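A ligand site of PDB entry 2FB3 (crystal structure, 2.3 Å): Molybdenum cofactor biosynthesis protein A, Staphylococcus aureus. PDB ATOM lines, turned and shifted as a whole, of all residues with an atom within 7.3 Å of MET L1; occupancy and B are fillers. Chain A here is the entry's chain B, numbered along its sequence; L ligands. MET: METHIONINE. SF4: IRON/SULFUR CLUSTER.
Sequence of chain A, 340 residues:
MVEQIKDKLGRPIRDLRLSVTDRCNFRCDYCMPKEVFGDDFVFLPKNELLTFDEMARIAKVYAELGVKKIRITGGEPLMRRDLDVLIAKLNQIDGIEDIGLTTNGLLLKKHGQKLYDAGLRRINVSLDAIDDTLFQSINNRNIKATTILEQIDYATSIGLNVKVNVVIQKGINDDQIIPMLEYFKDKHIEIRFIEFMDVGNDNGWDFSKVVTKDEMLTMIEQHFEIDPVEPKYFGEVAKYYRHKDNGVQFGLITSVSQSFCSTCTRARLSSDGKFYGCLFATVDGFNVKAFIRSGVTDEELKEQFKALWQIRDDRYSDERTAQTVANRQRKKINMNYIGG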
ATOM      1  N   ARG A  17     -10.624   7.779  -1.042  1.00  0.00           N
ATOM      2  CA  ARG A  17     -12.054   7.923  -1.266  1.00  0.00           C
ATOM      3  C   ARG A  17     -12.323   7.442  -2.645  1.00  0.00           C
ATOM      4  O   ARG A  17     -11.783   7.958  -3.607  1.00  0.00           O
ATOM      5  CB  ARG A  17     -12.499   9.368  -1.137  1.00  0.00           C
ATOM      6  CG  ARG A  17     -13.930   9.600  -1.601  1.00  0.00           C
ATOM      7  CD  ARG A  17     -14.377  11.045  -1.238  1.00  0.00           C
ATOM      8  NE  ARG A  17     -15.599  10.947  -0.441  1.00  0.00           N
ATOM      9  CZ  ARG A  17     -15.794  11.483   0.762  1.00  0.00           C
ATOM     10  NH1 ARG A  17     -14.857  12.247   1.339  1.00  0.00           N
ATOM     11  NH2 ARG A  17     -16.963  11.276   1.386  1.00  0.00           N
ATOM     12  N   SER A  19     -15.006   6.829  -5.524  1.00  0.00           N
ATOM     13  CA  SER A  19     -16.265   7.046  -6.218  1.00  0.00           C
ATOM     14  C   SER A  19     -16.531   5.960  -7.228  1.00  0.00           C
ATOM     15  O   SER A  19     -15.704   5.626  -8.088  1.00  0.00           O
ATOM     16  CB  SER A  19     -16.299   8.409  -6.901  1.00  0.00           C
ATOM     17  OG  SER A  19     -17.595   8.960  -6.792  1.00  0.00           O
ATOM     18  N   ARG A  23     -24.374   8.141 -10.264  1.00  0.00           N
ATOM     19  CA  ARG A  23     -25.842   8.158 -10.146  1.00  0.00           C
ATOM     20  C   ARG A  23     -26.350   8.227  -8.722  1.00  0.00           C
ATOM     21  O   ARG A  23     -25.609   7.972  -7.785  1.00  0.00           O
ATOM     22  CB  ARG A  23     -26.463   6.969 -10.856  1.00  0.00           C
ATOM     23  CG  ARG A  23     -26.090   6.863 -12.296  1.00  0.00           C
ATOM     24  CD  ARG A  23     -26.426   5.492 -12.728  1.00  0.00           C
ATOM     25  NE  ARG A  23     -26.563   5.365 -14.174  1.00  0.00           N
ATOM     26  CZ  ARG A  23     -27.597   5.828 -14.876  1.00  0.00           C
ATOM     27  NH1 ARG A  23     -28.585   6.485 -14.275  1.00  0.00           N
ATOM     28  NH2 ARG A  23     -27.630   5.622 -16.197  1.00  0.00           N
ATOM     29  N   CYS A  24     -27.614   8.586  -8.572  1.00  0.00           N
ATOM     30  CA  CYS A  24     -28.231   8.666  -7.255  1.00  0.00           C
ATOM     31  C   CYS A  24     -29.749   8.602  -7.353  1.00  0.00           C
ATOM     32  O   CYS A  24     -30.330   9.028  -8.348  1.00  0.00           O
ATOM     33  CB  CYS A  24     -27.781   9.925  -6.527  1.00  0.00           C
ATOM     34  SG  CYS A  24     -28.390  10.097  -4.819  1.00  0.00           S
ATOM     35  N   ASN A  25     -30.367   8.048  -6.316  1.00  0.00           N
ATOM     36  CA  ASN A  25     -31.817   7.920  -6.222  1.00  0.00           C
ATOM     37  C   ASN A  25     -32.453   9.074  -5.440  1.00  0.00           C
ATOM     38  O   ASN A  25     -33.618   8.994  -5.064  1.00  0.00           O
ATOM     39  CB  ASN A  25     -32.163   6.567  -5.579  1.00  0.00           C
ATOM     40  CG  ASN A  25     -31.267   6.235  -4.353  1.00  0.00           C
ATOM     41  OD1 ASN A  25     -30.532   7.076  -3.868  1.00  0.00           O
ATOM     42  ND2 ASN A  25     -31.382   5.008  -3.866  1.00  0.00           N
ATOM     43  N   PHE A  26     -31.654  10.125  -5.210  1.00  0.00           N
ATOM     44  CA  PHE A  26     -32.083  11.371  -4.554  1.00  0.00           C
ATOM     45  C   PHE A  26     -31.681  12.547  -5.443  1.00  0.00           C
ATOM     46  O   PHE A  26     -30.783  12.442  -6.288  1.00  0.00           O
ATOM     47  CB  PHE A  26     -31.301  11.601  -3.255  1.00  0.00           C
ATOM     48  CG  PHE A  26     -31.849  10.919  -2.037  1.00  0.00           C
ATOM     49  CD1 PHE A  26     -31.607  11.465  -0.776  1.00  0.00           C
ATOM     50  CD2 PHE A  26     -32.581   9.753  -2.112  1.00  0.00           C
ATOM     51  CE1 PHE A  26     -32.093  10.855   0.365  1.00  0.00           C
ATOM     52  CE2 PHE A  26     -33.061   9.131  -0.975  1.00  0.00           C
ATOM     53  CZ  PHE A  26     -32.827   9.658   0.252  1.00  0.00           C
ATOM     54  N   CYS A  28     -31.017  15.835  -3.756  1.00  0.00           N
ATOM     55  CA  CYS A  28     -30.722  16.875  -2.761  1.00  0.00           C
ATOM     56  C   CYS A  28     -30.146  18.078  -3.515  1.00  0.00           C
ATOM     57  O   CYS A  28     -29.336  17.913  -4.422  1.00  0.00           O
ATOM     58  CB  CYS A  28     -29.732  16.368  -1.670  1.00  0.00           C
ATOM     59  SG  CYS A  28     -30.194  14.771  -0.818  1.00  0.00           S
ATOM     60  N   TYR A  30     -28.297  20.848  -2.476  1.00  0.00           N
ATOM     61  CA  TYR A  30     -26.912  21.236  -2.223  1.00  0.00           C
ATOM     62  C   TYR A  30     -26.014  20.462  -3.191  1.00  0.00           C
ATOM     63  O   TYR A  30     -24.975  20.960  -3.633  1.00  0.00           O
ATOM     64  CB  TYR A  30     -26.516  20.869  -0.786  1.00  0.00           C
ATOM     65  CG  TYR A  30     -25.027  20.908  -0.458  1.00  0.00           C
ATOM     66  CD1 TYR A  30     -24.401  22.113  -0.098  1.00  0.00           C
ATOM     67  CD2 TYR A  30     -24.248  19.728  -0.474  1.00  0.00           C
ATOM     68  CE1 TYR A  30     -23.025  22.148   0.239  1.00  0.00           C
ATOM     69  CE2 TYR A  30     -22.873  19.750  -0.151  1.00  0.00           C
ATOM     70  CZ  TYR A  30     -22.268  20.966   0.213  1.00  0.00           C
ATOM     71  OH  TYR A  30     -20.929  21.016   0.540  1.00  0.00           O
ATOM     72  N   CYS A  31     -26.462  19.267  -3.529  1.00  0.00           N
ATOM     73  CA  CYS A  31     -25.603  18.251  -4.126  1.00  0.00           C
ATOM     74  C   CYS A  31     -25.969  17.935  -5.584  1.00  0.00           C
ATOM     75  O   CYS A  31     -25.206  18.265  -6.509  1.00  0.00           O
ATOM     76  CB  CYS A  31     -25.619  17.012  -3.231  1.00  0.00           C
ATOM     77  SG  CYS A  31     -24.713  15.613  -3.864  1.00  0.00           S
ATOM     78  N   MET A  32     -27.129  17.309  -5.796  1.00  0.00           N
ATOM     79  CA  MET A  32     -27.601  16.990  -7.155  1.00  0.00           C
ATOM     80  C   MET A  32     -28.979  17.597  -7.504  1.00  0.00           C
ATOM     81  O   MET A  32     -29.920  16.843  -7.777  1.00  0.00           O
ATOM     82  CB  MET A  32     -27.637  15.460  -7.382  1.00  0.00           C
ATOM     83  CG  MET A  32     -26.286  14.767  -7.403  1.00  0.00           C
ATOM     84  SD  MET A  32     -26.413  13.043  -7.945  1.00  0.00           S
ATOM     85  CE  MET A  32     -24.680  12.556  -7.975  1.00  0.00           C
ATOM     86  N   ILE A  72     -15.958   4.124   0.191  1.00  0.00           N
ATOM     87  CA  ILE A  72     -16.765   3.974  -1.030  1.00  0.00           C
ATOM     88  C   ILE A  72     -17.855   5.064  -1.040  1.00  0.00           C
ATOM     89  O   ILE A  72     -18.689   5.107  -0.122  1.00  0.00           O
ATOM     90  CB  ILE A  72     -17.435   2.552  -1.157  1.00  0.00           C
ATOM     91  CG1 ILE A  72     -16.369   1.448  -1.095  1.00  0.00           C
ATOM     92  CG2 ILE A  72     -18.255   2.385  -2.454  1.00  0.00           C
ATOM     93  CD1 ILE A  72     -15.104   1.775  -1.875  1.00  0.00           C
ATOM     94  N   THR A  73     -17.786   5.956  -2.041  1.00  0.00           N
ATOM     95  CA  THR A  73     -18.876   6.907  -2.365  1.00  0.00           C
ATOM     96  C   THR A  73     -19.382   6.910  -3.819  1.00  0.00           C
ATOM     97  O   THR A  73     -18.964   6.112  -4.676  1.00  0.00           O
ATOM     98  CB  THR A  73     -18.504   8.353  -2.060  1.00  0.00           C
ATOM     99  OG1 THR A  73     -17.090   8.563  -2.207  1.00  0.00           O
ATOM    100  CG2 THR A  73     -18.962   8.723  -0.667  1.00  0.00           C
ATOM    101  N   GLY A  74     -20.303   7.843  -4.086  1.00  0.00           N
ATOM    102  CA  GLY A  74     -20.699   8.223  -5.430  1.00  0.00           C
ATOM    103  C   GLY A  74     -20.988   9.710  -5.448  1.00  0.00           C
ATOM    104  O   GLY A  74     -20.149  10.511  -5.014  1.00  0.00           O
ATOM    105  N   GLY A  75     -22.181  10.122  -5.879  1.00  0.00           N
ATOM    106  CA  GLY A  75     -23.281   9.198  -6.172  1.00  0.00           C
ATOM    107  C   GLY A  75     -23.880   8.566  -4.943  1.00  0.00           C
ATOM    108  O   GLY A  75     -23.505   8.889  -3.802  1.00  0.00           O
ATOM    109  N   GLU A  76     -24.850   7.721  -5.178  1.00  0.00           N
ATOM    110  CA  GLU A  76     -25.218   6.647  -4.271  1.00  0.00           C
ATOM    111  C   GLU A  76     -24.381   5.441  -4.696  1.00  0.00           C
ATOM    112  O   GLU A  76     -24.555   4.930  -5.810  1.00  0.00           O
ATOM    113  CB  GLU A  76     -26.726   6.324  -4.350  1.00  0.00           C
ATOM    114  CG  GLU A  76     -27.244   5.280  -3.343  1.00  0.00           C
ATOM    115  CD  GLU A  76     -26.600   5.436  -1.949  1.00  0.00           C
ATOM    116  OE1 GLU A  76     -26.298   4.398  -1.328  1.00  0.00           O
ATOM    117  OE2 GLU A  76     -26.401   6.568  -1.467  1.00  0.00           O
ATOM    118  N   PRO A  77     -23.421   5.020  -3.843  1.00  0.00           N
ATOM    119  CA  PRO A  77     -22.669   3.763  -4.039  1.00  0.00           C
ATOM    120  C   PRO A  77     -23.549   2.531  -4.220  1.00  0.00           C
ATOM    121  O   PRO A  77     -23.220   1.674  -5.062  1.00  0.00           O
ATOM    122  CB  PRO A  77     -21.866   3.617  -2.742  1.00  0.00           C
ATOM    123  CG  PRO A  77     -22.481   4.604  -1.785  1.00  0.00           C
ATOM    124  CD  PRO A  77     -22.961   5.735  -2.628  1.00  0.00           C
ATOM    125  N   LEU A  78     -24.638   2.414  -3.454  1.00  0.00           N
ATOM    126  CA  LEU A  78     -25.564   1.267  -3.637  1.00  0.00           C
ATOM    127  C   LEU A  78     -26.258   1.223  -4.991  1.00  0.00           C
ATOM    128  O   LEU A  78     -26.884   0.222  -5.337  1.00  0.00           O
ATOM    129  CB  LEU A  78     -26.580   1.174  -2.492  1.00  0.00           C
ATOM    130  CG  LEU A  78     -25.957   0.882  -1.116  1.00  0.00           C
ATOM    131  CD1 LEU A  78     -26.970   0.844  -0.004  1.00  0.00           C
ATOM    132  CD2 LEU A  78     -25.262  -0.455  -1.179  1.00  0.00           C
ATOM    133  N   LEU A 101     -18.324   2.979   3.759  1.00  0.00           N
ATOM    134  CA  LEU A 101     -19.254   3.263   2.692  1.00  0.00           C
ATOM    135  C   LEU A 101     -20.147   4.362   3.182  1.00  0.00           C
ATOM    136  O   LEU A 101     -20.697   4.286   4.288  1.00  0.00           O
ATOM    137  CB  LEU A 101     -20.000   1.983   2.310  1.00  0.00           C
ATOM    138  CG  LEU A 101     -21.122   1.931   1.271  1.00  0.00           C
ATOM    139  CD1 LEU A 101     -20.949   0.703   0.446  1.00  0.00           C
ATOM    140  CD2 LEU A 101     -22.429   1.824   1.989  1.00  0.00           C
ATOM    141  N   THR A 102     -20.214   5.427   2.397  1.00  0.00           N
ATOM    142  CA  THR A 102     -21.127   6.555   2.658  1.00  0.00           C
ATOM    143  C   THR A 102     -22.372   6.378   1.794  1.00  0.00           C
ATOM    144  O   THR A 102     -22.276   6.369   0.563  1.00  0.00           O
ATOM    145  CB  THR A 102     -20.429   7.910   2.409  1.00  0.00           C
ATOM    146  OG1 THR A 102     -19.147   7.863   3.027  1.00  0.00           O
ATOM    147  CG2 THR A 102     -21.234   9.140   2.981  1.00  0.00           C
ATOM    148  N   THR A 103     -23.509   6.146   2.450  1.00  0.00           N
ATOM    149  CA  THR A 103     -24.811   6.050   1.783  1.00  0.00           C
ATOM    150  C   THR A 103     -25.914   7.017   2.329  1.00  0.00           C
ATOM    151  O   THR A 103     -25.820   7.491   3.477  1.00  0.00           O
ATOM    152  CB  THR A 103     -25.354   4.605   1.812  1.00  0.00           C
ATOM    153  OG1 THR A 103     -26.656   4.568   1.173  1.00  0.00           O
ATOM    154  CG2 THR A 103     -25.479   4.105   3.244  1.00  0.00           C
ATOM    155  N   ASN A 104     -26.918   7.327   1.492  1.00  0.00           N
ATOM    156  CA  ASN A 104     -28.198   7.898   1.960  1.00  0.00           C
ATOM    157  C   ASN A 104     -29.109   6.798   2.580  1.00  0.00           C
ATOM    158  O   ASN A 104     -30.118   7.114   3.205  1.00  0.00           O
ATOM    159  CB  ASN A 104     -28.944   8.668   0.845  1.00  0.00           C
ATOM    160  CG  ASN A 104     -29.386   7.760  -0.328  1.00  0.00           C
ATOM    161  OD1 ASN A 104     -29.791   6.628  -0.124  1.00  0.00           O
ATOM    162  ND2 ASN A 104     -29.294   8.266  -1.557  1.00  0.00           N
ATOM    163  N   GLY A 105     -28.732   5.531   2.386  1.00  0.00           N
ATOM    164  CA  GLY A 105     -29.333   4.419   3.131  1.00  0.00           C
ATOM    165  C   GLY A 105     -30.519   3.710   2.496  1.00  0.00           C
ATOM    166  O   GLY A 105     -30.899   2.600   2.914  1.00  0.00           O
ATOM    167  N   ASN A 124     -21.493   4.971   7.025  1.00  0.00           N
ATOM    168  CA  ASN A 124     -22.030   6.312   7.374  1.00  0.00           C
ATOM    169  C   ASN A 124     -23.322   6.558   6.553  1.00  0.00           C
ATOM    170  O   ASN A 124     -23.300   6.459   5.322  1.00  0.00           O
ATOM    171  CB  ASN A 124     -21.025   7.418   7.041  1.00  0.00           C
ATOM    172  CG  ASN A 124     -19.745   7.364   7.886  1.00  0.00           C
ATOM    173  OD1 ASN A 124     -18.718   6.837   7.460  1.00  0.00           O
ATOM    174  ND2 ASN A 124     -19.793   7.941   9.087  1.00  0.00           N
ATOM    175  N   VAL A 125     -24.439   6.833   7.230  1.00  0.00           N
ATOM    176  CA  VAL A 125     -25.714   7.148   6.546  1.00  0.00           C
ATOM    177  C   VAL A 125     -25.936   8.659   6.660  1.00  0.00           C
ATOM    178  O   VAL A 125     -26.011   9.205   7.771  1.00  0.00           O
ATOM    179  CB  VAL A 125     -26.931   6.351   7.116  1.00  0.00           C
ATOM    180  CG1 VAL A 125     -28.208   6.761   6.457  1.00  0.00           C
ATOM    181  CG2 VAL A 125     -26.747   4.860   6.896  1.00  0.00           C
ATOM    182  N   SER A 126     -25.957   9.353   5.517  1.00  0.00           N
ATOM    183  CA  SER A 126     -26.407  10.739   5.474  1.00  0.00           C
ATOM    184  C   SER A 126     -27.922  10.804   5.724  1.00  0.00           C
ATOM    185  O   SER A 126     -28.652   9.908   5.361  1.00  0.00           O
ATOM    186  CB  SER A 126     -26.051  11.412   4.158  1.00  0.00           C
ATOM    187  OG  SER A 126     -24.656  11.361   3.930  1.00  0.00           O
ATOM    188  N   LEU A 127     -28.366  11.858   6.383  1.00  0.00           N
ATOM    189  CA  LEU A 127     -29.771  12.009   6.711  1.00  0.00           C
ATOM    190  C   LEU A 127     -29.883  13.409   7.235  1.00  0.00           C
ATOM    191  O   LEU A 127     -29.706  13.636   8.428  1.00  0.00           O
ATOM    192  CB  LEU A 127     -30.186  10.972   7.759  1.00  0.00           C
ATOM    193  CG  LEU A 127     -31.592  11.021   8.367  1.00  0.00           C
ATOM    194  CD1 LEU A 127     -32.668  10.486   7.414  1.00  0.00           C
ATOM    195  CD2 LEU A 127     -31.556  10.216   9.640  1.00  0.00           C
ATOM    196  N   ASN A 165     -24.447  11.110   9.189  1.00  0.00           N
ATOM    197  CA  ASN A 165     -23.895  12.407   8.788  1.00  0.00           C
ATOM    198  C   ASN A 165     -24.974  13.452   8.465  1.00  0.00           C
ATOM    199  O   ASN A 165     -25.676  13.366   7.431  1.00  0.00           O
ATOM    200  CB  ASN A 165     -22.951  12.204   7.593  1.00  0.00           C
ATOM    201  CG  ASN A 165     -21.700  11.425   7.961  1.00  0.00           C
ATOM    202  OD1 ASN A 165     -20.834  11.918   8.675  1.00  0.00           O
ATOM    203  ND2 ASN A 165     -21.591  10.201   7.473  1.00  0.00           N
HETATM  204  N   MET L   1     -25.121   9.213  -1.436  1.00  0.00           N
HETATM  205  CA  MET L   1     -24.282   9.290  -0.196  1.00  0.00           C
HETATM  206  C   MET L   1     -24.795  10.326   0.807  1.00  0.00           C
HETATM  207  O   MET L   1     -25.288   9.972   1.892  1.00  0.00           O
HETATM  208  CB  MET L   1     -22.790   9.520  -0.519  1.00  0.00           C
HETATM  209  CG  MET L   1     -22.436  10.551  -1.611  1.00  0.00           C
HETATM  210  SD  MET L   1     -22.568  12.315  -1.178  1.00  0.00           S
HETATM  211  CE  MET L   1     -21.577  13.012  -2.523  1.00  0.00           C
HETATM  212  OXT MET L   1     -24.719  11.543   0.537  1.00  0.00           O
HETATM  213 FE1  SF4 L   2     -27.463  11.880  -3.603  1.00  0.00          FE
HETATM  214 FE2  SF4 L   2     -28.279  13.737  -2.042  1.00  0.00          FE
HETATM  215 FE3  SF4 L   2     -25.941  11.990  -1.492  1.00  0.00          FE
HETATM  216 FE4  SF4 L   2     -25.983  13.952  -3.111  1.00  0.00          FE
HETATM  217  S1  SF4 L   2     -26.378  14.058  -1.086  1.00  0.00           S
HETATM  218  S2  SF4 L   2     -25.298  11.930  -3.503  1.00  0.00           S
HETATM  219  S3  SF4 L   2     -27.884  13.940  -4.114  1.00  0.00           S
HETATM  220  S4  SF4 L   2     -28.072  11.665  -1.640  1.00  0.00           S
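The backbone carbonyl oxygen of Ile 72 sits at hydrogen-bond distance from the backbone NH of Thr 102.
The side-chain carboxylate (OE1) of Glu 76 sits at hydrogen-bond distance from the side-chain hydroxyl (OG1) of Thr 103 (2.5 Å).
O of Thr 103 sits at hydrogen-bond distance from N of Ser 126.
The side-chain carboxylate (OE2) of Glu 76 is in hydrogen-bond range of the backbone NH (N) of Asn 104, 3.1 Å away.
O of Asn 124 is in hydrogen-bond range of N of Thr 103, 2.9 Å away.
The backbone NH of Glu 76 sits at hydrogen-bond distance from the backbone carbonyl oxygen of Arg 23, at 2.7 Å.
O of Gly 74 lies close to OG of Ser 19 (3.5 Å).
The side-chain hydroxyl (OG1) of Thr 103 lies within hydrogen-bond range of the backbone NH (N) of Gly 105 (2.6 Å).
OXT of MET L1 binds FE3 of SF4 L2 (2.4 Å).
The backbone carbonyl oxygen (O) of Gly 75 is in hydrogen-bond range of a nitrogen (N) of MET L1 (2.9 Å).
The backbone NH (N) of Asn 104 lies within hydrogen-bond range of an oxygen (O) of MET L1, 3.1 Å away.
O of Thr 103 sits close to O of MET L1, at 3.0 Å.
SG of Cys 24 is bound to FE1 of SF4 L2, at 2.3 Å.
N of Cys 28 sits close to S3 of SF4 L2, 3.7 Å away.
The side-chain hydroxyl (OG) of Ser 126 lies within hydrogen-bond range of an oxygen (O) of MET L1, at 2.5 Å.
The side-chain carboxylate (OE2) of Glu 76 lies within salt-bridge range of a nitrogen (N) of MET L1 (2.9 Å).
An iron atom (FE2) of SF4 L2 is bound by the side-chain sulfur (SG) of Cys 28 (2.5 Å).
The side-chain amide nitrogen (ND2) of Asn 104 sits close to a sulfur (S4) of SF4 L2, at 3.6 Å.
An iron atom (FE4) of SF4 L2 is bound by the side-chain sulfur (SG) of Cys 31 (2.2 Å).
Residues that only touch MET L1: Thr 73, Gly 74 and Thr 102.
Of the 27 residues printed, 8 come within 4 Å of MET L1.
Along chain A the residues within 4 Å of MET L1 span positions 73 to 126.
The nearest printed residue that does not touch MET L1 is Pro 77 (4.3 Å).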
